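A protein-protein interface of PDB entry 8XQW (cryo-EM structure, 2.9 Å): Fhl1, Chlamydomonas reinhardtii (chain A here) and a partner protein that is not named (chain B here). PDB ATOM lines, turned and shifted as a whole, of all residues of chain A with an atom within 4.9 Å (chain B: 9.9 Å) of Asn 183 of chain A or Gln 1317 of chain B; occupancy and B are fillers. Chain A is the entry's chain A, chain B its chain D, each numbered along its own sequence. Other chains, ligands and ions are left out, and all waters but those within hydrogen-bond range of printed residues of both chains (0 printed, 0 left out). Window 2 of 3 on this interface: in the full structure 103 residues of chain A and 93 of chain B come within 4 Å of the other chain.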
ATOM      1  N   PRO A 178     -16.835   6.381   0.478  1.00  0.00           N
ATOM      2  CA  PRO A 178     -17.780   7.031  -0.438  1.00  0.00           C
ATOM      3  C   PRO A 178     -17.384   8.430  -0.853  1.00  0.00           C
ATOM      4  O   PRO A 178     -17.614   8.797  -2.012  1.00  0.00           O
ATOM      5  CB  PRO A 178     -19.083   7.039   0.365  1.00  0.00           C
ATOM      6  CG  PRO A 178     -18.943   5.906   1.298  1.00  0.00           C
ATOM      7  CD  PRO A 178     -17.503   5.862   1.679  1.00  0.00           C
ATOM      8  N   ALA A 179     -16.786   9.214   0.046  1.00  0.00           N
ATOM      9  CA  ALA A 179     -16.432  10.592  -0.282  1.00  0.00           C
ATOM     10  C   ALA A 179     -15.659  10.668  -1.586  1.00  0.00           C
ATOM     11  O   ALA A 179     -16.018  11.443  -2.480  1.00  0.00           O
ATOM     12  CB  ALA A 179     -15.622  11.212   0.852  1.00  0.00           C
ATOM     13  N   ILE A 180     -14.625   9.833  -1.728  1.00  0.00           N
ATOM     14  CA  ILE A 180     -13.787   9.827  -2.924  1.00  0.00           C
ATOM     15  C   ILE A 180     -14.630   9.926  -4.183  1.00  0.00           C
ATOM     16  O   ILE A 180     -14.312  10.686  -5.103  1.00  0.00           O
ATOM     17  CB  ILE A 180     -12.908   8.565  -2.946  1.00  0.00           C
ATOM     18  CG1 ILE A 180     -11.869   8.626  -1.835  1.00  0.00           C
ATOM     19  CG2 ILE A 180     -12.237   8.407  -4.289  1.00  0.00           C
ATOM     20  CD1 ILE A 180     -10.876   7.503  -1.893  1.00  0.00           C
ATOM     21  N   PHE A 181     -15.725   9.178  -4.241  1.00  0.00           N
ATOM     22  CA  PHE A 181     -16.577   9.250  -5.415  1.00  0.00           C
ATOM     23  C   PHE A 181     -17.529  10.430  -5.328  1.00  0.00           C
ATOM     24  O   PHE A 181     -17.582  11.259  -6.238  1.00  0.00           O
ATOM     25  CB  PHE A 181     -17.349   7.949  -5.578  1.00  0.00           C
ATOM     26  CG  PHE A 181     -18.474   8.034  -6.552  1.00  0.00           C
ATOM     27  CD1 PHE A 181     -18.230   8.088  -7.901  1.00  0.00           C
ATOM     28  CD2 PHE A 181     -19.776   8.035  -6.118  1.00  0.00           C
ATOM     29  CE1 PHE A 181     -19.264   8.154  -8.796  1.00  0.00           C
ATOM     30  CE2 PHE A 181     -20.809   8.103  -7.006  1.00  0.00           C
ATOM     31  CZ  PHE A 181     -20.554   8.163  -8.346  1.00  0.00           C
ATOM     32  N   TRP A 182     -18.258  10.539  -4.219  1.00  0.00           N
ATOM     33  CA  TRP A 182     -19.333  11.518  -4.133  1.00  0.00           C
ATOM     34  C   TRP A 182     -18.803  12.927  -4.322  1.00  0.00           C
ATOM     35  O   TRP A 182     -19.376  13.720  -5.074  1.00  0.00           O
ATOM     36  CB  TRP A 182     -20.050  11.373  -2.798  1.00  0.00           C
ATOM     37  CG  TRP A 182     -20.653  12.616  -2.289  1.00  0.00           C
ATOM     38  CD1 TRP A 182     -20.090  13.499  -1.427  1.00  0.00           C
ATOM     39  CD2 TRP A 182     -21.957  13.112  -2.579  1.00  0.00           C
ATOM     40  NE1 TRP A 182     -20.958  14.526  -1.168  1.00  0.00           N
ATOM     41  CE2 TRP A 182     -22.114  14.310  -1.866  1.00  0.00           C
ATOM     42  CE3 TRP A 182     -23.006  12.662  -3.375  1.00  0.00           C
ATOM     43  CZ2 TRP A 182     -23.272  15.066  -1.931  1.00  0.00           C
ATOM     44  CZ3 TRP A 182     -24.154  13.413  -3.438  1.00  0.00           C
ATOM     45  CH2 TRP A 182     -24.280  14.599  -2.722  1.00  0.00           C
ATOM     46  N   ASN A 183     -17.686  13.244  -3.670  1.00  0.00           N
ATOM     47  CA  ASN A 183     -17.078  14.558  -3.831  1.00  0.00           C
ATOM     48  C   ASN A 183     -16.928  14.943  -5.292  1.00  0.00           C
ATOM     49  O   ASN A 183     -17.197  16.090  -5.655  1.00  0.00           O
ATOM     50  CB  ASN A 183     -15.721  14.593  -3.141  1.00  0.00           C
ATOM     51  CG  ASN A 183     -15.815  15.054  -1.716  1.00  0.00           C
ATOM     52  OD1 ASN A 183     -16.855  15.533  -1.282  1.00  0.00           O
ATOM     53  ND2 ASN A 183     -14.728  14.919  -0.975  1.00  0.00           N
ATOM     54  N   LYS A 184     -16.517  14.008  -6.151  1.00  0.00           N
ATOM     55  CA  LYS A 184     -16.415  14.329  -7.570  1.00  0.00           C
ATOM     56  C   LYS A 184     -17.784  14.597  -8.163  1.00  0.00           C
ATOM     57  O   LYS A 184     -18.000  15.637  -8.789  1.00  0.00           O
ATOM     58  CB  LYS A 184     -15.733  13.198  -8.330  1.00  0.00           C
ATOM     59  CG  LYS A 184     -14.277  13.040  -8.012  1.00  0.00           C
ATOM     60  CD  LYS A 184     -13.456  14.101  -8.684  1.00  0.00           C
ATOM     61  CE  LYS A 184     -12.006  13.972  -8.286  1.00  0.00           C
ATOM     62  NZ  LYS A 184     -11.158  15.013  -8.922  1.00  0.00           N
ATOM     63  N   LEU A 185     -18.722  13.679  -7.954  1.00  0.00           N
ATOM     64  CA  LEU A 185     -20.052  13.823  -8.528  1.00  0.00           C
ATOM     65  C   LEU A 185     -20.643  15.182  -8.195  1.00  0.00           C
ATOM     66  O   LEU A 185     -21.126  15.896  -9.079  1.00  0.00           O
ATOM     67  CB  LEU A 185     -20.946  12.703  -8.015  1.00  0.00           C
ATOM     68  CG  LEU A 185     -22.400  12.721  -8.443  1.00  0.00           C
ATOM     69  CD1 LEU A 185     -22.486  12.522  -9.923  1.00  0.00           C
ATOM     70  CD2 LEU A 185     -23.144  11.634  -7.720  1.00  0.00           C
ATOM     71  N   LEU A 186     -20.569  15.576  -6.928  1.00  0.00           N
ATOM     72  CA  LEU A 186     -21.148  16.841  -6.501  1.00  0.00           C
ATOM     73  C   LEU A 186     -20.497  18.043  -7.164  1.00  0.00           C
ATOM     74  O   LEU A 186     -21.178  19.047  -7.380  1.00  0.00           O
ATOM     75  CB  LEU A 186     -21.040  16.966  -4.991  1.00  0.00           C
ATOM     76  CG  LEU A 186     -21.682  18.217  -4.416  1.00  0.00           C
ATOM     77  CD1 LEU A 186     -23.130  17.954  -4.109  1.00  0.00           C
ATOM     78  CD2 LEU A 186     -20.942  18.637  -3.183  1.00  0.00           C
ATOM     79  N   ASP A 187     -19.212  17.976  -7.501  1.00  0.00           N
ATOM     80  CA  ASP A 187     -18.596  19.108  -8.181  1.00  0.00           C
ATOM     81  C   ASP A 187     -19.148  19.323  -9.572  1.00  0.00           C
ATOM     82  O   ASP A 187     -18.968  20.406 -10.128  1.00  0.00           O
ATOM     83  CB  ASP A 187     -17.085  18.936  -8.284  1.00  0.00           C
ATOM     84  CG  ASP A 187     -16.441  18.664  -6.953  1.00  0.00           C
ATOM     85  OD1 ASP A 187     -17.123  18.844  -5.924  1.00  0.00           O
ATOM     86  OD2 ASP A 187     -15.252  18.281  -6.931  1.00  0.00           O
ATOM     87  N   LYS B1250     -22.051  17.033   7.350  1.00  0.00           N
ATOM     88  CA  LYS B1250     -21.182  16.118   8.076  1.00  0.00           C
ATOM     89  C   LYS B1250     -20.257  16.878   9.013  1.00  0.00           C
ATOM     90  O   LYS B1250     -19.967  16.414  10.121  1.00  0.00           O
ATOM     91  CB  LYS B1250     -20.375  15.269   7.098  1.00  0.00           C
ATOM     92  CG  LYS B1250     -21.224  14.401   6.201  1.00  0.00           C
ATOM     93  CD  LYS B1250     -21.870  13.269   6.973  1.00  0.00           C
ATOM     94  CE  LYS B1250     -22.483  12.248   6.032  1.00  0.00           C
ATOM     95  NZ  LYS B1250     -23.443  12.877   5.088  1.00  0.00           N
ATOM     96  N   LEU B1254     -20.280  15.971  12.995  1.00  0.00           N
ATOM     97  CA  LEU B1254     -19.048  15.553  13.647  1.00  0.00           C
ATOM     98  C   LEU B1254     -18.951  16.104  15.060  1.00  0.00           C
ATOM     99  O   LEU B1254     -18.341  15.475  15.930  1.00  0.00           O
ATOM    100  CB  LEU B1254     -17.843  15.999  12.829  1.00  0.00           C
ATOM    101  CG  LEU B1254     -17.318  14.992  11.816  1.00  0.00           C
ATOM    102  CD1 LEU B1254     -15.965  15.442  11.320  1.00  0.00           C
ATOM    103  CD2 LEU B1254     -17.243  13.609  12.425  1.00  0.00           C
ATOM    104  N   LYS B1301     -11.001   7.499  13.355  1.00  0.00           N
ATOM    105  CA  LYS B1301     -11.359   8.106  12.078  1.00  0.00           C
ATOM    106  C   LYS B1301     -12.148   9.387  12.286  1.00  0.00           C
ATOM    107  O   LYS B1301     -11.862  10.409  11.647  1.00  0.00           O
ATOM    108  CB  LYS B1301     -12.157   7.128  11.223  1.00  0.00           C
ATOM    109  CG  LYS B1301     -11.361   6.530  10.081  1.00  0.00           C
ATOM    110  CD  LYS B1301     -10.013   6.029  10.564  1.00  0.00           C
ATOM    111  CE  LYS B1301      -9.340   5.147   9.529  1.00  0.00           C
ATOM    112  NZ  LYS B1301      -8.086   4.535  10.055  1.00  0.00           N
ATOM    113  N   LYS B1304      -9.732  12.035  13.286  1.00  0.00           N
ATOM    114  CA  LYS B1304      -8.975  12.545  12.147  1.00  0.00           C
ATOM    115  C   LYS B1304      -9.798  13.539  11.343  1.00  0.00           C
ATOM    116  O   LYS B1304      -9.290  14.592  10.939  1.00  0.00           O
ATOM    117  CB  LYS B1304      -8.536  11.395  11.250  1.00  0.00           C
ATOM    118  CG  LYS B1304      -7.419  10.564  11.807  1.00  0.00           C
ATOM    119  CD  LYS B1304      -6.986   9.525  10.802  1.00  0.00           C
ATOM    120  CE  LYS B1304      -5.876   8.658  11.349  1.00  0.00           C
ATOM    121  NZ  LYS B1304      -5.485   7.605  10.376  1.00  0.00           N
ATOM    122  N   GLN B1305     -11.059  13.206  11.077  1.00  0.00           N
ATOM    123  CA  GLN B1305     -11.916  14.122  10.336  1.00  0.00           C
ATOM    124  C   GLN B1305     -12.044  15.454  11.058  1.00  0.00           C
ATOM    125  O   GLN B1305     -11.954  16.521  10.436  1.00  0.00           O
ATOM    126  CB  GLN B1305     -13.289  13.501  10.120  1.00  0.00           C
ATOM    127  CG  GLN B1305     -13.251  12.156   9.449  1.00  0.00           C
ATOM    128  CD  GLN B1305     -13.294  12.266   7.952  1.00  0.00           C
ATOM    129  OE1 GLN B1305     -13.777  13.256   7.409  1.00  0.00           O
ATOM    130  NE2 GLN B1305     -12.779  11.257   7.270  1.00  0.00           N
ATOM    131  N   LYS B1306     -12.261  15.411  12.373  1.00  0.00           N
ATOM    132  CA  LYS B1306     -12.292  16.642  13.155  1.00  0.00           C
ATOM    133  C   LYS B1306     -11.019  17.445  12.949  1.00  0.00           C
ATOM    134  O   LYS B1306     -11.063  18.635  12.611  1.00  0.00           O
ATOM    135  CB  LYS B1306     -12.479  16.316  14.634  1.00  0.00           C
ATOM    136  CG  LYS B1306     -13.916  16.128  15.062  1.00  0.00           C
ATOM    137  CD  LYS B1306     -14.042  16.176  16.568  1.00  0.00           C
ATOM    138  CE  LYS B1306     -15.436  16.594  16.988  1.00  0.00           C
ATOM    139  NZ  LYS B1306     -15.450  17.161  18.366  1.00  0.00           N
ATOM    140  N   LEU B1307      -9.866  16.801  13.141  1.00  0.00           N
ATOM    141  CA  LEU B1307      -8.598  17.511  13.034  1.00  0.00           C
ATOM    142  C   LEU B1307      -8.457  18.183  11.682  1.00  0.00           C
ATOM    143  O   LEU B1307      -8.024  19.334  11.593  1.00  0.00           O
ATOM    144  CB  LEU B1307      -7.445  16.548  13.261  1.00  0.00           C
ATOM    145  CG  LEU B1307      -7.274  16.068  14.689  1.00  0.00           C
ATOM    146  CD1 LEU B1307      -6.543  14.754  14.697  1.00  0.00           C
ATOM    147  CD2 LEU B1307      -6.516  17.113  15.460  1.00  0.00           C
ATOM    148  N   ASN B1308      -8.825  17.475  10.617  1.00  0.00           N
ATOM    149  CA  ASN B1308      -8.673  18.029   9.279  1.00  0.00           C
ATOM    150  C   ASN B1308      -9.593  19.217   9.067  1.00  0.00           C
ATOM    151  O   ASN B1308      -9.195  20.208   8.449  1.00  0.00           O
ATOM    152  CB  ASN B1308      -8.951  16.960   8.236  1.00  0.00           C
ATOM    153  CG  ASN B1308      -8.777  17.469   6.840  1.00  0.00           C
ATOM    154  OD1 ASN B1308      -7.659  17.591   6.350  1.00  0.00           O
ATOM    155  ND2 ASN B1308      -9.882  17.769   6.182  1.00  0.00           N
ATOM    156  N   TYR B1309     -10.827  19.137   9.566  1.00  0.00           N
ATOM    157  CA  TYR B1309     -11.709  20.295   9.482  1.00  0.00           C
ATOM    158  C   TYR B1309     -11.187  21.450  10.318  1.00  0.00           C
ATOM    159  O   TYR B1309     -11.589  22.596  10.104  1.00  0.00           O
ATOM    160  CB  TYR B1309     -13.111  19.931   9.945  1.00  0.00           C
ATOM    161  CG  TYR B1309     -13.966  19.288   8.894  1.00  0.00           C
ATOM    162  CD1 TYR B1309     -14.129  19.873   7.653  1.00  0.00           C
ATOM    163  CD2 TYR B1309     -14.620  18.096   9.146  1.00  0.00           C
ATOM    164  CE1 TYR B1309     -14.918  19.285   6.692  1.00  0.00           C
ATOM    165  CE2 TYR B1309     -15.407  17.501   8.194  1.00  0.00           C
ATOM    166  CZ  TYR B1309     -15.554  18.097   6.969  1.00  0.00           C
ATOM    167  OH  TYR B1309     -16.345  17.495   6.020  1.00  0.00           O
ATOM    168  N   TYR B1313      -3.859  19.052   9.229  1.00  0.00           N
ATOM    169  CA  TYR B1313      -3.639  17.614   9.250  1.00  0.00           C
ATOM    170  C   TYR B1313      -3.359  17.144   7.830  1.00  0.00           C
ATOM    171  O   TYR B1313      -3.967  17.622   6.872  1.00  0.00           O
ATOM    172  CB  TYR B1313      -4.848  16.879   9.835  1.00  0.00           C
ATOM    173  CG  TYR B1313      -4.522  15.516  10.384  1.00  0.00           C
ATOM    174  CD1 TYR B1313      -3.604  15.360  11.405  1.00  0.00           C
ATOM    175  CD2 TYR B1313      -5.135  14.384   9.878  1.00  0.00           C
ATOM    176  CE1 TYR B1313      -3.303  14.117  11.903  1.00  0.00           C
ATOM    177  CE2 TYR B1313      -4.839  13.136  10.369  1.00  0.00           C
ATOM    178  CZ  TYR B1313      -3.923  13.007  11.381  1.00  0.00           C
ATOM    179  OH  TYR B1313      -3.631  11.757  11.871  1.00  0.00           O
ATOM    180  N   LEU B1314      -2.432  16.192   7.690  1.00  0.00           N
ATOM    181  CA  LEU B1314      -1.770  16.009   6.402  1.00  0.00           C
ATOM    182  C   LEU B1314      -2.031  14.667   5.723  1.00  0.00           C
ATOM    183  O   LEU B1314      -1.260  14.290   4.842  1.00  0.00           O
ATOM    184  CB  LEU B1314      -0.261  16.220   6.544  1.00  0.00           C
ATOM    185  CG  LEU B1314       0.269  17.544   5.989  1.00  0.00           C
ATOM    186  CD1 LEU B1314      -0.673  18.686   6.300  1.00  0.00           C
ATOM    187  CD2 LEU B1314       1.654  17.843   6.528  1.00  0.00           C
ATOM    188  N   ASN B1315      -3.053  13.912   6.116  1.00  0.00           N
ATOM    189  CA  ASN B1315      -3.529  12.874   5.204  1.00  0.00           C
ATOM    190  C   ASN B1315      -4.984  12.496   5.420  1.00  0.00           C
ATOM    191  O   ASN B1315      -5.264  11.520   6.117  1.00  0.00           O
ATOM    192  CB  ASN B1315      -2.673  11.617   5.338  1.00  0.00           C
ATOM    193  CG  ASN B1315      -1.803  11.378   4.132  1.00  0.00           C
ATOM    194  OD1 ASN B1315      -2.251  10.820   3.135  1.00  0.00           O
ATOM    195  ND2 ASN B1315      -0.546  11.793   4.215  1.00  0.00           N
ATOM    196  N   VAL B1316      -5.908  13.196   4.767  1.00  0.00           N
ATOM    197  CA  VAL B1316      -7.334  12.900   4.851  1.00  0.00           C
ATOM    198  C   VAL B1316      -8.042  13.641   3.733  1.00  0.00           C
ATOM    199  O   VAL B1316      -7.539  14.636   3.208  1.00  0.00           O
ATOM    200  CB  VAL B1316      -7.965  13.282   6.212  1.00  0.00           C
ATOM    201  CG1 VAL B1316      -7.996  12.102   7.157  1.00  0.00           C
ATOM    202  CG2 VAL B1316      -7.199  14.414   6.828  1.00  0.00           C
ATOM    203  N   GLN B1317      -9.270  13.210   3.432  1.00  0.00           N
ATOM    204  CA  GLN B1317     -10.098  13.906   2.420  1.00  0.00           C
ATOM    205  C   GLN B1317     -11.458  14.232   3.043  1.00  0.00           C
ATOM    206  O   GLN B1317     -12.132  13.289   3.481  1.00  0.00           O
ATOM    207  CB  GLN B1317     -10.335  13.013   1.209  1.00  0.00           C
ATOM    208  CG  GLN B1317     -11.074  13.706   0.073  1.00  0.00           C
ATOM    209  CD  GLN B1317     -11.973  12.771  -0.703  1.00  0.00           C
ATOM    210  OE1 GLN B1317     -12.364  11.705  -0.219  1.00  0.00           O
ATOM    211  NE2 GLN B1317     -12.302  13.163  -1.925  1.00  0.00           N
ATOM    212  N   SER B1318     -11.848  15.505   3.065  1.00  0.00           N
ATOM    213  CA  SER B1318     -13.137  15.925   3.665  1.00  0.00           C
ATOM    214  C   SER B1318     -14.306  15.567   2.751  1.00  0.00           C
ATOM    215  O   SER B1318     -14.059  15.344   1.562  1.00  0.00           O
ATOM    216  CB  SER B1318     -13.129  17.385   3.873  1.00  0.00           C
ATOM    217  OG  SER B1318     -12.985  18.052   2.628  1.00  0.00           O
ATOM    218  N   GLU B1319     -15.531  15.544   3.273  1.00  0.00           N
ATOM    219  CA  GLU B1319     -16.721  15.313   2.412  1.00  0.00           C
ATOM    220  C   GLU B1319     -17.410  16.666   2.198  1.00  0.00           C
ATOM    221  O   GLU B1319     -17.344  17.506   3.112  1.00  0.00           O
ATOM    222  CB  GLU B1319     -17.676  14.274   2.992  1.00  0.00           C
ATOM    223  CG  GLU B1319     -19.125  14.743   3.026  1.00  0.00           C
ATOM    224  CD  GLU B1319     -20.125  13.622   3.207  1.00  0.00           C
ATOM    225  OE1 GLU B1319     -19.776  12.670   3.933  1.00  0.00           O
ATOM    226  OE2 GLU B1319     -21.237  13.691   2.645  1.00  0.00           O
ATOM    227  N   HIS B1320     -18.013  16.878   1.028  1.00  0.00           N
ATOM    228  CA  HIS B1320     -18.630  18.192   0.718  1.00  0.00           C
ATOM    229  C   HIS B1320     -20.142  18.069   0.885  1.00  0.00           C
ATOM    230  O   HIS B1320     -20.657  16.940   0.917  1.00  0.00           O
ATOM    231  CB  HIS B1320     -18.179  18.646  -0.670  1.00  0.00           C
ATOM    232  CG  HIS B1320     -16.699  18.732  -0.814  1.00  0.00           C
ATOM    233  ND1 HIS B1320     -15.860  18.976   0.251  1.00  0.00           N
ATOM    234  CD2 HIS B1320     -15.910  18.608  -1.885  1.00  0.00           C
ATOM    235  CE1 HIS B1320     -14.608  18.993  -0.175  1.00  0.00           C
ATOM    236  NE2 HIS B1320     -14.615  18.772  -1.470  1.00  0.00           N
ATOM    237  N   ASN B1321     -20.840  19.197   0.977  1.00  0.00           N
ATOM    238  CA  ASN B1321     -22.295  19.139   1.264  1.00  0.00           C
ATOM    239  C   ASN B1321     -23.104  19.909   0.225  1.00  0.00           C
ATOM    240  O   ASN B1321     -22.541  20.813  -0.407  1.00  0.00           O
ATOM    241  CB  ASN B1321     -22.586  19.696   2.653  1.00  0.00           C
ATOM    242  CG  ASN B1321     -22.506  21.202   2.716  1.00  0.00           C
ATOM    243  OD1 ASN B1321     -21.425  21.776   2.550  1.00  0.00           O
ATOM    244  ND2 ASN B1321     -23.628  21.859   2.963  1.00  0.00           N
ATOM    245  N   VAL B1322     -24.376  19.557   0.055  1.00  0.00           N
ATOM    246  CA  VAL B1322     -25.246  20.325  -0.822  1.00  0.00           C
ATOM    247  C   VAL B1322     -25.487  21.700  -0.220  1.00  0.00           C
ATOM    248  O   VAL B1322     -25.711  21.837   0.987  1.00  0.00           O
ATOM    249  CB  VAL B1322     -26.572  19.579  -1.030  1.00  0.00           C
ATOM    250  CG1 VAL B1322     -27.495  20.382  -1.913  1.00  0.00           C
ATOM    251  CG2 VAL B1322     -26.317  18.211  -1.611  1.00  0.00           C
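ND2 of Asn 183 of chain A sits close to NE2 of Gln 1317 of chain B. N of Ile 180 of chain A lies within hydrogen-bond range of OE1 of Gln 1317 of chain B. ND2 of Asn 183 of chain A sits at hydrogen-bond distance from O of Ser 1318 of chain B (2.7 Å). The backbone carbonyl oxygen (O) of His 1320 of chain B sits at hydrogen-bond distance from the indole nitrogen (NE1) of Trp 182 of chain A (3.2 Å). The side-chain amide oxygen of Asn 183 of chain A is in hydrogen-bond range of the backbone NH of His 1320 of chain B, at 2.9 Å.
The backbone carbonyl oxygen of Glu 1319 of chain B lies within hydrogen-bond range of the side-chain hydroxyl of Tyr 1309 of chain B (3.1 Å). NZ of Lys 1250 of chain B lies within salt-bridge range of OE2 of Glu 1319 of chain B (3.4 Å).
Gln 1317 of chain B touches Ala 179 of chain A. Glu 1319 of chain B touches Trp 182 of chain A. C of Glu 1319 of chain B touches OD1 of Asn 183 of chain A (3.7 Å). CD2 of Leu 186 of chain A touches CB of His 1320 of chain B, at 3.7 Å. Leu 186 of chain A touches Asn 1321 of chain B (CD2 to O, 3.9 Å).
Asn 183 of chain A touches just these residues of chain B: Gln 1317 (3.1 Å), Ser 1318 (2.7 Å), Glu 1319 (3.7 Å) and His 1320 (2.9 Å). Printed residues of chain A within 4 Å of Gln 1317 of chain B: Ala 179 (3.5 Å), Ile 180 (3.3 Å) and Asn 183 (3.1 Å). Of the printed residues of chain B, Ala 179 of chain A touches Gln 1317 (3.5 Å). Printed residues of chain A within 4 Å of Ser 1318 of chain B: Asn 183 (2.7 Å). Of the printed residues of chain A, Asn 1321 of chain B touches Leu 186. Printed residues of chain A within 4 Å of Glu 1319 of chain B: Trp 182 (3.9 Å) and Asn 183 (3.7 Å). Lys 1301 of chain B touches none of the printed residues of chain A. Pro 178 of chain A touches none of the printed residues of chain B. The nearest residue of chain B that does not touch Asn 183 of chain A is Asn 1321 of chain B (5.9 Å). The nearest printed residue of chain A that does not touch Gln 1317 of chain B is Phe 181 of chain A (5.7 Å).
Of the 10 printed residues of chain A, 5 touch a printed residue of chain B. Of the 19 printed residues of chain B, 5 touch a printed residue of chain A. Hydrophobic or aromatic side chains of chain B that line the printed part of chain A: His 1320. Among the printed residues, 10 pairs touch across the chains.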
